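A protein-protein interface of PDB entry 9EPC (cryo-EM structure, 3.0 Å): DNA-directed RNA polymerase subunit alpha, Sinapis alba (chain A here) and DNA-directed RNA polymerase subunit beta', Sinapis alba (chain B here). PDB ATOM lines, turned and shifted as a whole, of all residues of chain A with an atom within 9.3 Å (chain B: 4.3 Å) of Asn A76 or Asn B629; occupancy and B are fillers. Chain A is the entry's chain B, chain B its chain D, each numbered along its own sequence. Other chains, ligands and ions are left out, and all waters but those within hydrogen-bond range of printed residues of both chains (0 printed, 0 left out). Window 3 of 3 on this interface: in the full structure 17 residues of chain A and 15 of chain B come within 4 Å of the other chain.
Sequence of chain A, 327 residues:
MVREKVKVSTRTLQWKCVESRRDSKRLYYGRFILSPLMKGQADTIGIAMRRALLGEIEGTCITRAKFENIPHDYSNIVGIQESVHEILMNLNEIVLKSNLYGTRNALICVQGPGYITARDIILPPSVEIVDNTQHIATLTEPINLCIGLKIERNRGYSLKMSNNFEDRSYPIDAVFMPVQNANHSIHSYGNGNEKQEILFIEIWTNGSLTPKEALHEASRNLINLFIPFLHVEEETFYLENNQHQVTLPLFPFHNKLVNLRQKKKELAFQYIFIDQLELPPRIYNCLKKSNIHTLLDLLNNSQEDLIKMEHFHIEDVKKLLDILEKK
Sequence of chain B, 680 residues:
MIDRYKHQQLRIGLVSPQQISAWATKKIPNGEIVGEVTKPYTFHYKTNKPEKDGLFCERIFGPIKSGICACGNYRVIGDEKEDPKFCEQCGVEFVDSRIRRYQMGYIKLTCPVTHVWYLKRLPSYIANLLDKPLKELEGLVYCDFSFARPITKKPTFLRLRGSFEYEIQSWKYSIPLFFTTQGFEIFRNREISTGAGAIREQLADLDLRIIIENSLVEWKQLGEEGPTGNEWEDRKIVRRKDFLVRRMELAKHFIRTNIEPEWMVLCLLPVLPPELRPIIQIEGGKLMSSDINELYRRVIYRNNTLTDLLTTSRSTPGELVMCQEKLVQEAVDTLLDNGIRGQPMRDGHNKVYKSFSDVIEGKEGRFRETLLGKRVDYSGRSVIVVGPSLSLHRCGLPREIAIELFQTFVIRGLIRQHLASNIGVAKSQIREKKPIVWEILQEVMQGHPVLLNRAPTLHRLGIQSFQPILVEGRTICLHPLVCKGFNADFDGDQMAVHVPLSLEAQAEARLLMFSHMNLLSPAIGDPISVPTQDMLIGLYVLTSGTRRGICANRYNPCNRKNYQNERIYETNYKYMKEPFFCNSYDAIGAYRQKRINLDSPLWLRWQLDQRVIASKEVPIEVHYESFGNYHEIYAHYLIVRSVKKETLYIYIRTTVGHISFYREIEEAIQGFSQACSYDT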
ATOM      1  N   PHE A  67       2.655 -22.899  -0.123  1.00  0.00           N
ATOM      2  CA  PHE A  67       3.349 -24.182  -0.198  1.00  0.00           C
ATOM      3  C   PHE A  67       2.450 -25.160  -0.939  1.00  0.00           C
ATOM      4  O   PHE A  67       1.642 -25.874  -0.345  1.00  0.00           O
ATOM      5  CB  PHE A  67       3.713 -24.682   1.193  1.00  0.00           C
ATOM      6  CG  PHE A  67       4.884 -23.972   1.798  1.00  0.00           C
ATOM      7  CD1 PHE A  67       4.719 -22.761   2.445  1.00  0.00           C
ATOM      8  CD2 PHE A  67       6.152 -24.513   1.717  1.00  0.00           C
ATOM      9  CE1 PHE A  67       5.799 -22.106   3.000  1.00  0.00           C
ATOM     10  CE2 PHE A  67       7.237 -23.861   2.268  1.00  0.00           C
ATOM     11  CZ  PHE A  67       7.059 -22.657   2.911  1.00  0.00           C
ATOM     12  N   ILE A  70       1.807 -29.441  -0.564  1.00  0.00           N
ATOM     13  CA  ILE A  70       2.245 -29.764   0.785  1.00  0.00           C
ATOM     14  C   ILE A  70       1.063 -29.585   1.728  1.00  0.00           C
ATOM     15  O   ILE A  70       0.767 -28.474   2.168  1.00  0.00           O
ATOM     16  CB  ILE A  70       3.437 -28.891   1.217  1.00  0.00           C
ATOM     17  CG1 ILE A  70       4.623 -29.112   0.279  1.00  0.00           C
ATOM     18  CG2 ILE A  70       3.836 -29.205   2.649  1.00  0.00           C
ATOM     19  CD1 ILE A  70       5.123 -30.536   0.259  1.00  0.00           C
ATOM     20  N   PRO A  71       0.351 -30.662   2.052  1.00  0.00           N
ATOM     21  CA  PRO A  71      -0.717 -30.593   3.058  1.00  0.00           C
ATOM     22  C   PRO A  71      -0.257 -30.833   4.489  1.00  0.00           C
ATOM     23  O   PRO A  71      -1.110 -31.004   5.365  1.00  0.00           O
ATOM     24  CB  PRO A  71      -1.653 -31.720   2.606  1.00  0.00           C
ATOM     25  CG  PRO A  71      -0.725 -32.744   2.046  1.00  0.00           C
ATOM     26  CD  PRO A  71       0.409 -31.981   1.398  1.00  0.00           C
ATOM     27  N   HIS A  72       1.054 -30.856   4.739  1.00  0.00           N
ATOM     28  CA  HIS A  72       1.555 -31.156   6.077  1.00  0.00           C
ATOM     29  C   HIS A  72       1.087 -30.116   7.086  1.00  0.00           C
ATOM     30  O   HIS A  72       0.633 -30.460   8.183  1.00  0.00           O
ATOM     31  CB  HIS A  72       3.082 -31.231   6.056  1.00  0.00           C
ATOM     32  CG  HIS A  72       3.620 -32.397   5.288  1.00  0.00           C
ATOM     33  ND1 HIS A  72       4.964 -32.554   5.022  1.00  0.00           N
ATOM     34  CD2 HIS A  72       2.999 -33.464   4.734  1.00  0.00           C
ATOM     35  CE1 HIS A  72       5.146 -33.667   4.334  1.00  0.00           C
ATOM     36  NE2 HIS A  72       3.969 -34.239   4.147  1.00  0.00           N
ATOM     37  N   ASP A  73       1.196 -28.836   6.731  1.00  0.00           N
ATOM     38  CA  ASP A  73       0.817 -27.718   7.593  1.00  0.00           C
ATOM     39  C   ASP A  73       1.560 -27.736   8.927  1.00  0.00           C
ATOM     40  O   ASP A  73       1.111 -27.123   9.901  1.00  0.00           O
ATOM     41  CB  ASP A  73      -0.698 -27.688   7.828  1.00  0.00           C
ATOM     42  CG  ASP A  73      -1.209 -26.300   8.162  1.00  0.00           C
ATOM     43  OD1 ASP A  73      -0.392 -25.356   8.184  1.00  0.00           O
ATOM     44  OD2 ASP A  73      -2.425 -26.154   8.400  1.00  0.00           O
ATOM     45  N   TYR A  74       2.692 -28.433   8.993  1.00  0.00           N
ATOM     46  CA  TYR A  74       3.501 -28.473  10.197  1.00  0.00           C
ATOM     47  C   TYR A  74       4.608 -27.425  10.117  1.00  0.00           C
ATOM     48  O   TYR A  74       4.779 -26.736   9.109  1.00  0.00           O
ATOM     49  CB  TYR A  74       4.093 -29.866  10.409  1.00  0.00           C
ATOM     50  CG  TYR A  74       3.097 -30.995  10.298  1.00  0.00           C
ATOM     51  CD1 TYR A  74       1.967 -31.034  11.104  1.00  0.00           C
ATOM     52  CD2 TYR A  74       3.297 -32.035   9.402  1.00  0.00           C
ATOM     53  CE1 TYR A  74       1.057 -32.070  11.007  1.00  0.00           C
ATOM     54  CE2 TYR A  74       2.395 -33.073   9.297  1.00  0.00           C
ATOM     55  CZ  TYR A  74       1.277 -33.087  10.102  1.00  0.00           C
ATOM     56  OH  TYR A  74       0.376 -34.122  10.002  1.00  0.00           O
ATOM     57  N   SER A  75       5.379 -27.306  11.198  1.00  0.00           N
ATOM     58  CA  SER A  75       6.491 -26.367  11.215  1.00  0.00           C
ATOM     59  C   SER A  75       7.658 -26.836  10.358  1.00  0.00           C
ATOM     60  O   SER A  75       8.484 -26.011   9.953  1.00  0.00           O
ATOM     61  CB  SER A  75       6.962 -26.137  12.652  1.00  0.00           C
ATOM     62  OG  SER A  75       8.070 -25.255  12.690  1.00  0.00           O
ATOM     63  N   ASN A  76       7.747 -28.133  10.075  1.00  0.00           N
ATOM     64  CA  ASN A  76       8.824 -28.676   9.264  1.00  0.00           C
ATOM     65  C   ASN A  76       8.257 -29.700   8.293  1.00  0.00           C
ATOM     66  O   ASN A  76       7.210 -30.304   8.536  1.00  0.00           O
ATOM     67  CB  ASN A  76       9.918 -29.316  10.128  1.00  0.00           C
ATOM     68  CG  ASN A  76      10.684 -28.298  10.943  1.00  0.00           C
ATOM     69  OD1 ASN A  76      10.177 -27.767  11.930  1.00  0.00           O
ATOM     70  ND2 ASN A  76      11.918 -28.025  10.538  1.00  0.00           N
ATOM     71  N   ILE A  77       8.966 -29.887   7.184  1.00  0.00           N
ATOM     72  CA  ILE A  77       8.592 -30.857   6.166  1.00  0.00           C
ATOM     73  C   ILE A  77       9.802 -31.721   5.849  1.00  0.00           C
ATOM     74  O   ILE A  77      10.951 -31.301   6.016  1.00  0.00           O
ATOM     75  CB  ILE A  77       8.056 -30.177   4.889  1.00  0.00           C
ATOM     76  CG1 ILE A  77       9.024 -29.093   4.418  1.00  0.00           C
ATOM     77  CG2 ILE A  77       6.673 -29.598   5.135  1.00  0.00           C
ATOM     78  CD1 ILE A  77       8.509 -28.283   3.253  1.00  0.00           C
ATOM     79  N   VAL A  78       9.535 -32.944   5.388  1.00  0.00           N
ATOM     80  CA  VAL A  78      10.609 -33.888   5.118  1.00  0.00           C
ATOM     81  C   VAL A  78      11.420 -33.426   3.914  1.00  0.00           C
ATOM     82  O   VAL A  78      10.896 -32.811   2.975  1.00  0.00           O
ATOM     83  CB  VAL A  78      10.047 -35.305   4.899  1.00  0.00           C
ATOM     84  CG1 VAL A  78       9.362 -35.800   6.161  1.00  0.00           C
ATOM     85  CG2 VAL A  78       9.083 -35.320   3.726  1.00  0.00           C
ATOM     86  N   GLY A  79      12.720 -33.715   3.947  1.00  0.00           N
ATOM     87  CA  GLY A  79      13.613 -33.368   2.866  1.00  0.00           C
ATOM     88  C   GLY A  79      14.172 -31.965   2.913  1.00  0.00           C
ATOM     89  O   GLY A  79      15.095 -31.659   2.148  1.00  0.00           O
ATOM     90  N   ILE A  80      13.655 -31.103   3.783  1.00  0.00           N
ATOM     91  CA  ILE A  80      14.105 -29.721   3.896  1.00  0.00           C
ATOM     92  C   ILE A  80      14.611 -29.510   5.313  1.00  0.00           C
ATOM     93  O   ILE A  80      13.873 -29.732   6.280  1.00  0.00           O
ATOM     94  CB  ILE A  80      12.988 -28.719   3.559  1.00  0.00           C
ATOM     95  CG1 ILE A  80      12.586 -28.821   2.087  1.00  0.00           C
ATOM     96  CG2 ILE A  80      13.432 -27.306   3.882  1.00  0.00           C
ATOM     97  CD1 ILE A  80      11.507 -29.840   1.799  1.00  0.00           C
ATOM     98  N   GLN A  81      15.868 -29.085   5.437  1.00  0.00           N
ATOM     99  CA  GLN A  81      16.432 -28.828   6.757  1.00  0.00           C
ATOM    100  C   GLN A  81      15.748 -27.643   7.426  1.00  0.00           C
ATOM    101  O   GLN A  81      15.391 -27.704   8.608  1.00  0.00           O
ATOM    102  CB  GLN A  81      17.937 -28.591   6.647  1.00  0.00           C
ATOM    103  CG  GLN A  81      18.580 -28.122   7.940  1.00  0.00           C
ATOM    104  CD  GLN A  81      20.088 -28.029   7.842  1.00  0.00           C
ATOM    105  OE1 GLN A  81      20.691 -28.514   6.885  1.00  0.00           O
ATOM    106  NE2 GLN A  81      20.707 -27.398   8.833  1.00  0.00           N
ATOM    107  N   GLU A  82      15.555 -26.556   6.686  1.00  0.00           N
ATOM    108  CA  GLU A  82      14.954 -25.361   7.257  1.00  0.00           C
ATOM    109  C   GLU A  82      13.485 -25.595   7.588  1.00  0.00           C
ATOM    110  O   GLU A  82      12.768 -26.309   6.883  1.00  0.00           O
ATOM    111  CB  GLU A  82      15.086 -24.178   6.297  1.00  0.00           C
ATOM    112  CG  GLU A  82      16.474 -23.556   6.243  1.00  0.00           C
ATOM    113  CD  GLU A  82      17.469 -24.396   5.470  1.00  0.00           C
ATOM    114  OE1 GLU A  82      17.044 -25.352   4.788  1.00  0.00           O
ATOM    115  OE2 GLU A  82      18.679 -24.097   5.543  1.00  0.00           O
ATOM    116  N   SER A  83      13.041 -24.980   8.678  1.00  0.00           N
ATOM    117  CA  SER A  83      11.639 -25.033   9.042  1.00  0.00           C
ATOM    118  C   SER A  83      10.822 -24.155   8.099  1.00  0.00           C
ATOM    119  O   SER A  83      11.354 -23.334   7.347  1.00  0.00           O
ATOM    120  CB  SER A  83      11.443 -24.587  10.489  1.00  0.00           C
ATOM    121  OG  SER A  83      11.894 -23.257  10.672  1.00  0.00           O
ATOM    122  N   VAL A  84       9.501 -24.337   8.145  1.00  0.00           N
ATOM    123  CA  VAL A  84       8.618 -23.525   7.315  1.00  0.00           C
ATOM    124  C   VAL A  84       8.754 -22.054   7.679  1.00  0.00           C
ATOM    125  O   VAL A  84       8.808 -21.184   6.803  1.00  0.00           O
ATOM    126  CB  VAL A  84       7.164 -24.011   7.448  1.00  0.00           C
ATOM    127  CG1 VAL A  84       6.233 -23.089   6.691  1.00  0.00           C
ATOM    128  CG2 VAL A  84       7.039 -25.433   6.935  1.00  0.00           C
ATOM    129  N   HIS A  85       8.818 -21.754   8.977  1.00  0.00           N
ATOM    130  CA  HIS A  85       8.973 -20.369   9.409  1.00  0.00           C
ATOM    131  C   HIS A  85      10.302 -19.790   8.941  1.00  0.00           C
ATOM    132  O   HIS A  85      10.374 -18.617   8.557  1.00  0.00           O
ATOM    133  CB  HIS A  85       8.851 -20.280  10.927  1.00  0.00           C
ATOM    134  CG  HIS A  85       8.927 -18.885  11.458  1.00  0.00           C
ATOM    135  ND1 HIS A  85       9.960 -18.450  12.259  1.00  0.00           N
ATOM    136  CD2 HIS A  85       8.098 -17.827  11.306  1.00  0.00           C
ATOM    137  CE1 HIS A  85       9.763 -17.184  12.578  1.00  0.00           C
ATOM    138  NE2 HIS A  85       8.641 -16.781  12.010  1.00  0.00           N
ATOM    139  N   GLU A  86      11.369 -20.590   8.973  1.00  0.00           N
ATOM    140  CA  GLU A  86      12.665 -20.099   8.519  1.00  0.00           C
ATOM    141  C   GLU A  86      12.699 -19.898   7.011  1.00  0.00           C
ATOM    142  O   GLU A  86      13.400 -19.005   6.526  1.00  0.00           O
ATOM    143  CB  GLU A  86      13.776 -21.052   8.951  1.00  0.00           C
ATOM    144  CG  GLU A  86      14.307 -20.800  10.354  1.00  0.00           C
ATOM    145  CD  GLU A  86      15.050 -19.481  10.483  1.00  0.00           C
ATOM    146  OE1 GLU A  86      14.391 -18.422  10.553  1.00  0.00           O
ATOM    147  OE2 GLU A  86      16.298 -19.503  10.510  1.00  0.00           O
ATOM    148  N   ILE A  87      11.967 -20.719   6.256  1.00  0.00           N
ATOM    149  CA  ILE A  87      11.895 -20.519   4.812  1.00  0.00           C
ATOM    150  C   ILE A  87      11.260 -19.173   4.499  1.00  0.00           C
ATOM    151  O   ILE A  87      11.729 -18.438   3.623  1.00  0.00           O
ATOM    152  CB  ILE A  87      11.131 -21.678   4.148  1.00  0.00           C
ATOM    153  CG1 ILE A  87      11.959 -22.960   4.212  1.00  0.00           C
ATOM    154  CG2 ILE A  87      10.795 -21.337   2.709  1.00  0.00           C
ATOM    155  CD1 ILE A  87      11.294 -24.145   3.561  1.00  0.00           C
ATOM    156  N   TYR A 170       0.973 -18.392   3.555  1.00  0.00           N
ATOM    157  CA  TYR A 170       1.561 -17.781   4.738  1.00  0.00           C
ATOM    158  C   TYR A 170       2.048 -16.381   4.402  1.00  0.00           C
ATOM    159  O   TYR A 170       2.941 -16.237   3.558  1.00  0.00           O
ATOM    160  CB  TYR A 170       2.710 -18.624   5.262  1.00  0.00           C
ATOM    161  CG  TYR A 170       2.311 -20.035   5.635  1.00  0.00           C
ATOM    162  CD1 TYR A 170       0.995 -20.347   5.949  1.00  0.00           C
ATOM    163  CD2 TYR A 170       3.249 -21.053   5.670  1.00  0.00           C
ATOM    164  CE1 TYR A 170       0.626 -21.630   6.287  1.00  0.00           C
ATOM    165  CE2 TYR A 170       2.888 -22.341   6.009  1.00  0.00           C
ATOM    166  CZ  TYR A 170       1.577 -22.624   6.315  1.00  0.00           C
ATOM    167  OH  TYR A 170       1.217 -23.907   6.652  1.00  0.00           O
ATOM    168  N   HIS B 623       7.528 -26.267  23.625  1.00  0.00           N
ATOM    169  CA  HIS B 623       6.605 -26.863  22.662  1.00  0.00           C
ATOM    170  C   HIS B 623       7.362 -27.941  21.901  1.00  0.00           C
ATOM    171  O   HIS B 623       8.053 -27.659  20.921  1.00  0.00           O
ATOM    172  CB  HIS B 623       6.040 -25.805  21.725  1.00  0.00           C
ATOM    173  CG  HIS B 623       5.171 -24.800  22.409  1.00  0.00           C
ATOM    174  ND1 HIS B 623       4.842 -23.590  21.841  1.00  0.00           N
ATOM    175  CD2 HIS B 623       4.561 -24.828  23.617  1.00  0.00           C
ATOM    176  CE1 HIS B 623       4.067 -22.914  22.669  1.00  0.00           C
ATOM    177  NE2 HIS B 623       3.882 -23.642  23.755  1.00  0.00           N
ATOM    178  N   TYR B 624       7.219 -29.180  22.350  1.00  0.00           N
ATOM    179  CA  TYR B 624       7.960 -30.315  21.808  1.00  0.00           C
ATOM    180  C   TYR B 624       7.084 -30.994  20.760  1.00  0.00           C
ATOM    181  O   TYR B 624       6.144 -31.716  21.096  1.00  0.00           O
ATOM    182  CB  TYR B 624       8.339 -31.269  22.933  1.00  0.00           C
ATOM    183  CG  TYR B 624       9.577 -32.093  22.689  1.00  0.00           C
ATOM    184  CD1 TYR B 624      10.009 -32.378  21.404  1.00  0.00           C
ATOM    185  CD2 TYR B 624      10.313 -32.591  23.751  1.00  0.00           C
ATOM    186  CE1 TYR B 624      11.140 -33.132  21.188  1.00  0.00           C
ATOM    187  CE2 TYR B 624      11.441 -33.346  23.545  1.00  0.00           C
ATOM    188  CZ  TYR B 624      11.850 -33.615  22.262  1.00  0.00           C
ATOM    189  OH  TYR B 624      12.980 -34.369  22.058  1.00  0.00           O
ATOM    190  N   GLU B 625       7.391 -30.757  19.489  1.00  0.00           N
ATOM    191  CA  GLU B 625       6.642 -31.394  18.416  1.00  0.00           C
ATOM    192  C   GLU B 625       7.030 -32.860  18.291  1.00  0.00           C
ATOM    193  O   GLU B 625       8.130 -33.271  18.669  1.00  0.00           O
ATOM    194  CB  GLU B 625       6.881 -30.675  17.091  1.00  0.00           C
ATOM    195  CG  GLU B 625       6.515 -29.204  17.109  1.00  0.00           C
ATOM    196  CD  GLU B 625       6.758 -28.527  15.778  1.00  0.00           C
ATOM    197  OE1 GLU B 625       7.017 -29.239  14.786  1.00  0.00           O
ATOM    198  OE2 GLU B 625       6.692 -27.282  15.723  1.00  0.00           O
ATOM    199  N   PHE B 627       7.811 -34.547  15.782  1.00  0.00           N
ATOM    200  CA  PHE B 627       8.802 -34.840  14.758  1.00  0.00           C
ATOM    201  C   PHE B 627      10.225 -34.535  15.198  1.00  0.00           C
ATOM    202  O   PHE B 627      11.150 -34.680  14.392  1.00  0.00           O
ATOM    203  CB  PHE B 627       8.481 -34.068  13.477  1.00  0.00           C
ATOM    204  CG  PHE B 627       7.338 -34.644  12.698  1.00  0.00           C
ATOM    205  CD1 PHE B 627       6.960 -35.963  12.877  1.00  0.00           C
ATOM    206  CD2 PHE B 627       6.642 -33.870  11.787  1.00  0.00           C
ATOM    207  CE1 PHE B 627       5.909 -36.500  12.162  1.00  0.00           C
ATOM    208  CE2 PHE B 627       5.590 -34.402  11.068  1.00  0.00           C
ATOM    209  CZ  PHE B 627       5.223 -35.719  11.256  1.00  0.00           C
ATOM    210  N   GLY B 628      10.428 -34.117  16.444  1.00  0.00           N
ATOM    211  CA  GLY B 628      11.746 -33.864  16.982  1.00  0.00           C
ATOM    212  C   GLY B 628      12.070 -32.401  17.190  1.00  0.00           C
ATOM    213  O   GLY B 628      12.956 -32.087  17.993  1.00  0.00           O
ATOM    214  N   ASN B 629      11.390 -31.501  16.489  1.00  0.00           N
ATOM    215  CA  ASN B 629      11.600 -30.078  16.714  1.00  0.00           C
ATOM    216  C   ASN B 629      10.920 -29.654  18.006  1.00  0.00           C
ATOM    217  O   ASN B 629       9.747 -29.963  18.230  1.00  0.00           O
ATOM    218  CB  ASN B 629      11.050 -29.268  15.544  1.00  0.00           C
ATOM    219  CG  ASN B 629      11.713 -29.618  14.235  1.00  0.00           C
ATOM    220  OD1 ASN B 629      11.321 -30.570  13.564  1.00  0.00           O
ATOM    221  ND2 ASN B 629      12.724 -28.844  13.862  1.00  0.00           N
ATOM    222  N   TYR B 630      11.652 -28.949  18.862  1.00  0.00           N
ATOM    223  CA  TYR B 630      11.078 -28.418  20.087  1.00  0.00           C
ATOM    224  C   TYR B 630      11.476 -26.962  20.249  1.00  0.00           C
ATOM    225  O   TYR B 630      12.653 -26.615  20.111  1.00  0.00           O
ATOM    226  CB  TYR B 630      11.498 -29.234  21.315  1.00  0.00           C
ATOM    227  CG  TYR B 630      12.983 -29.356  21.553  1.00  0.00           C
ATOM    228  CD1 TYR B 630      13.732 -30.323  20.901  1.00  0.00           C
ATOM    229  CD2 TYR B 630      13.627 -28.533  22.462  1.00  0.00           C
ATOM    230  CE1 TYR B 630      15.084 -30.448  21.130  1.00  0.00           C
ATOM    231  CE2 TYR B 630      14.979 -28.651  22.696  1.00  0.00           C
ATOM    232  CZ  TYR B 630      15.702 -29.612  22.028  1.00  0.00           C
ATOM    233  OH  TYR B 630      17.052 -29.732  22.258  1.00  0.00           O
ATOM    234  N   ARG B 641      15.268 -25.650  18.799  1.00  0.00           N
ATOM    235  CA  ARG B 641      16.179 -26.767  18.614  1.00  0.00           C
ATOM    236  C   ARG B 641      15.436 -27.947  18.004  1.00  0.00           C
ATOM    237  O   ARG B 641      14.209 -27.962  17.905  1.00  0.00           O
ATOM    238  CB  ARG B 641      16.823 -27.171  19.941  1.00  0.00           C
ATOM    239  CG  ARG B 641      17.613 -26.069  20.606  1.00  0.00           C
ATOM    240  CD  ARG B 641      18.701 -26.634  21.501  1.00  0.00           C
ATOM    241  NE  ARG B 641      18.164 -27.312  22.672  1.00  0.00           N
ATOM    242  CZ  ARG B 641      17.981 -26.731  23.849  1.00  0.00           C
ATOM    243  NH1 ARG B 641      18.274 -25.456  24.042  1.00  0.00           N
ATOM    244  NH2 ARG B 641      17.494 -27.447  24.857  1.00  0.00           N
ATOM    245  N   SER B 642      16.203 -28.948  17.584  1.00  0.00           N
ATOM    246  CA  SER B 642      15.638 -30.144  16.986  1.00  0.00           C
ATOM    247  C   SER B 642      16.444 -31.354  17.427  1.00  0.00           C
ATOM    248  O   SER B 642      17.602 -31.241  17.832  1.00  0.00           O
ATOM    249  CB  SER B 642      15.611 -30.055  15.457  1.00  0.00           C
ATOM    250  OG  SER B 642      15.078 -31.239  14.893  1.00  0.00           O
ATOM    251  N   LYS B 645      18.202 -32.605  13.818  1.00  0.00           N
ATOM    252  CA  LYS B 645      19.220 -31.665  13.373  1.00  0.00           C
ATOM    253  C   LYS B 645      19.789 -30.913  14.575  1.00  0.00           C
ATOM    254  O   LYS B 645      19.489 -31.220  15.730  1.00  0.00           O
ATOM    255  CB  LYS B 645      18.626 -30.711  12.336  1.00  0.00           C
ATOM    256  CG  LYS B 645      17.912 -31.419  11.198  1.00  0.00           C
ATOM    257  CD  LYS B 645      16.975 -30.478  10.461  1.00  0.00           C
ATOM    258  CE  LYS B 645      15.860 -29.991  11.372  1.00  0.00           C
ATOM    259  NZ  LYS B 645      14.923 -29.074  10.669  1.00  0.00           N
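ND2 of Asn B629 sits close to OD1 of Asn A76 (3.4 Å).
The side-chain amino group (NZ) of Lys B645 lies close to the side-chain amide nitrogen (ND2) of Asn A76, 3.2 Å away.
The backbone carbonyl oxygen of Gln A81 is in hydrogen-bond range of the side-chain amino group of Lys B645.
OD1 of Asn A76 sits close to OG of Ser A75.
The backbone NH (N) of Val A84 sits at hydrogen-bond distance from the backbone carbonyl oxygen (O) of Ser A75 (2.7 Å).
Tyr A74 touches Phe B627 (CD2 to CE2, 3.7 Å).
Ser A75 touches Glu B625 (CB to OE2, 3.3 Å).
Of the printed residues of chain B, Tyr A74 touches Phe B627 (3.7 Å).
Of the printed residues of chain B, Ser A75 touches Glu B625 (3.3 Å).
Of chain B, only Asn B629 and Lys B645 come within 4 Å of Asn A76.
Of the printed residues of chain B, Gln A81 touches Lys B645 (2.5 Å).
Of chain A, only Ser A75 comes within 4 Å of Glu B625.
Printed residues of chain A within 4 Å of Phe B627: Tyr A74 (3.7 Å).
Gly B628 touches none of the printed residues of chain A.
Of the printed residues of chain A, Asn B629 touches Asn A76.
Printed residues of chain A within 4 Å of Lys B645: Asn A76 and Gln A81.
The nearest printed residue of chain B that does not touch Asn A76 is Glu B625 (4.5 Å).
The nearest residue of chain A that does not touch Asn B629 is Ser A83 (5.6 Å).
The nearest printed residue of chain B that does not touch Tyr A74 is Glu B625 (5.3 Å).
Printed residues of chain A that touch a printed residue of chain B: Tyr A74, Ser A75, Asn A76 and Gln A81.
Hydrophobic or aromatic side chains of chain A within 4 Å of the printed part of chain B: Tyr A74.
Among the printed residues, 5 pairs touch across the chains.
Among the printed residues, no Asp or Glu carboxylate lies within 4 Å of a Lys or Arg side-chain nitrogen of the other chain.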
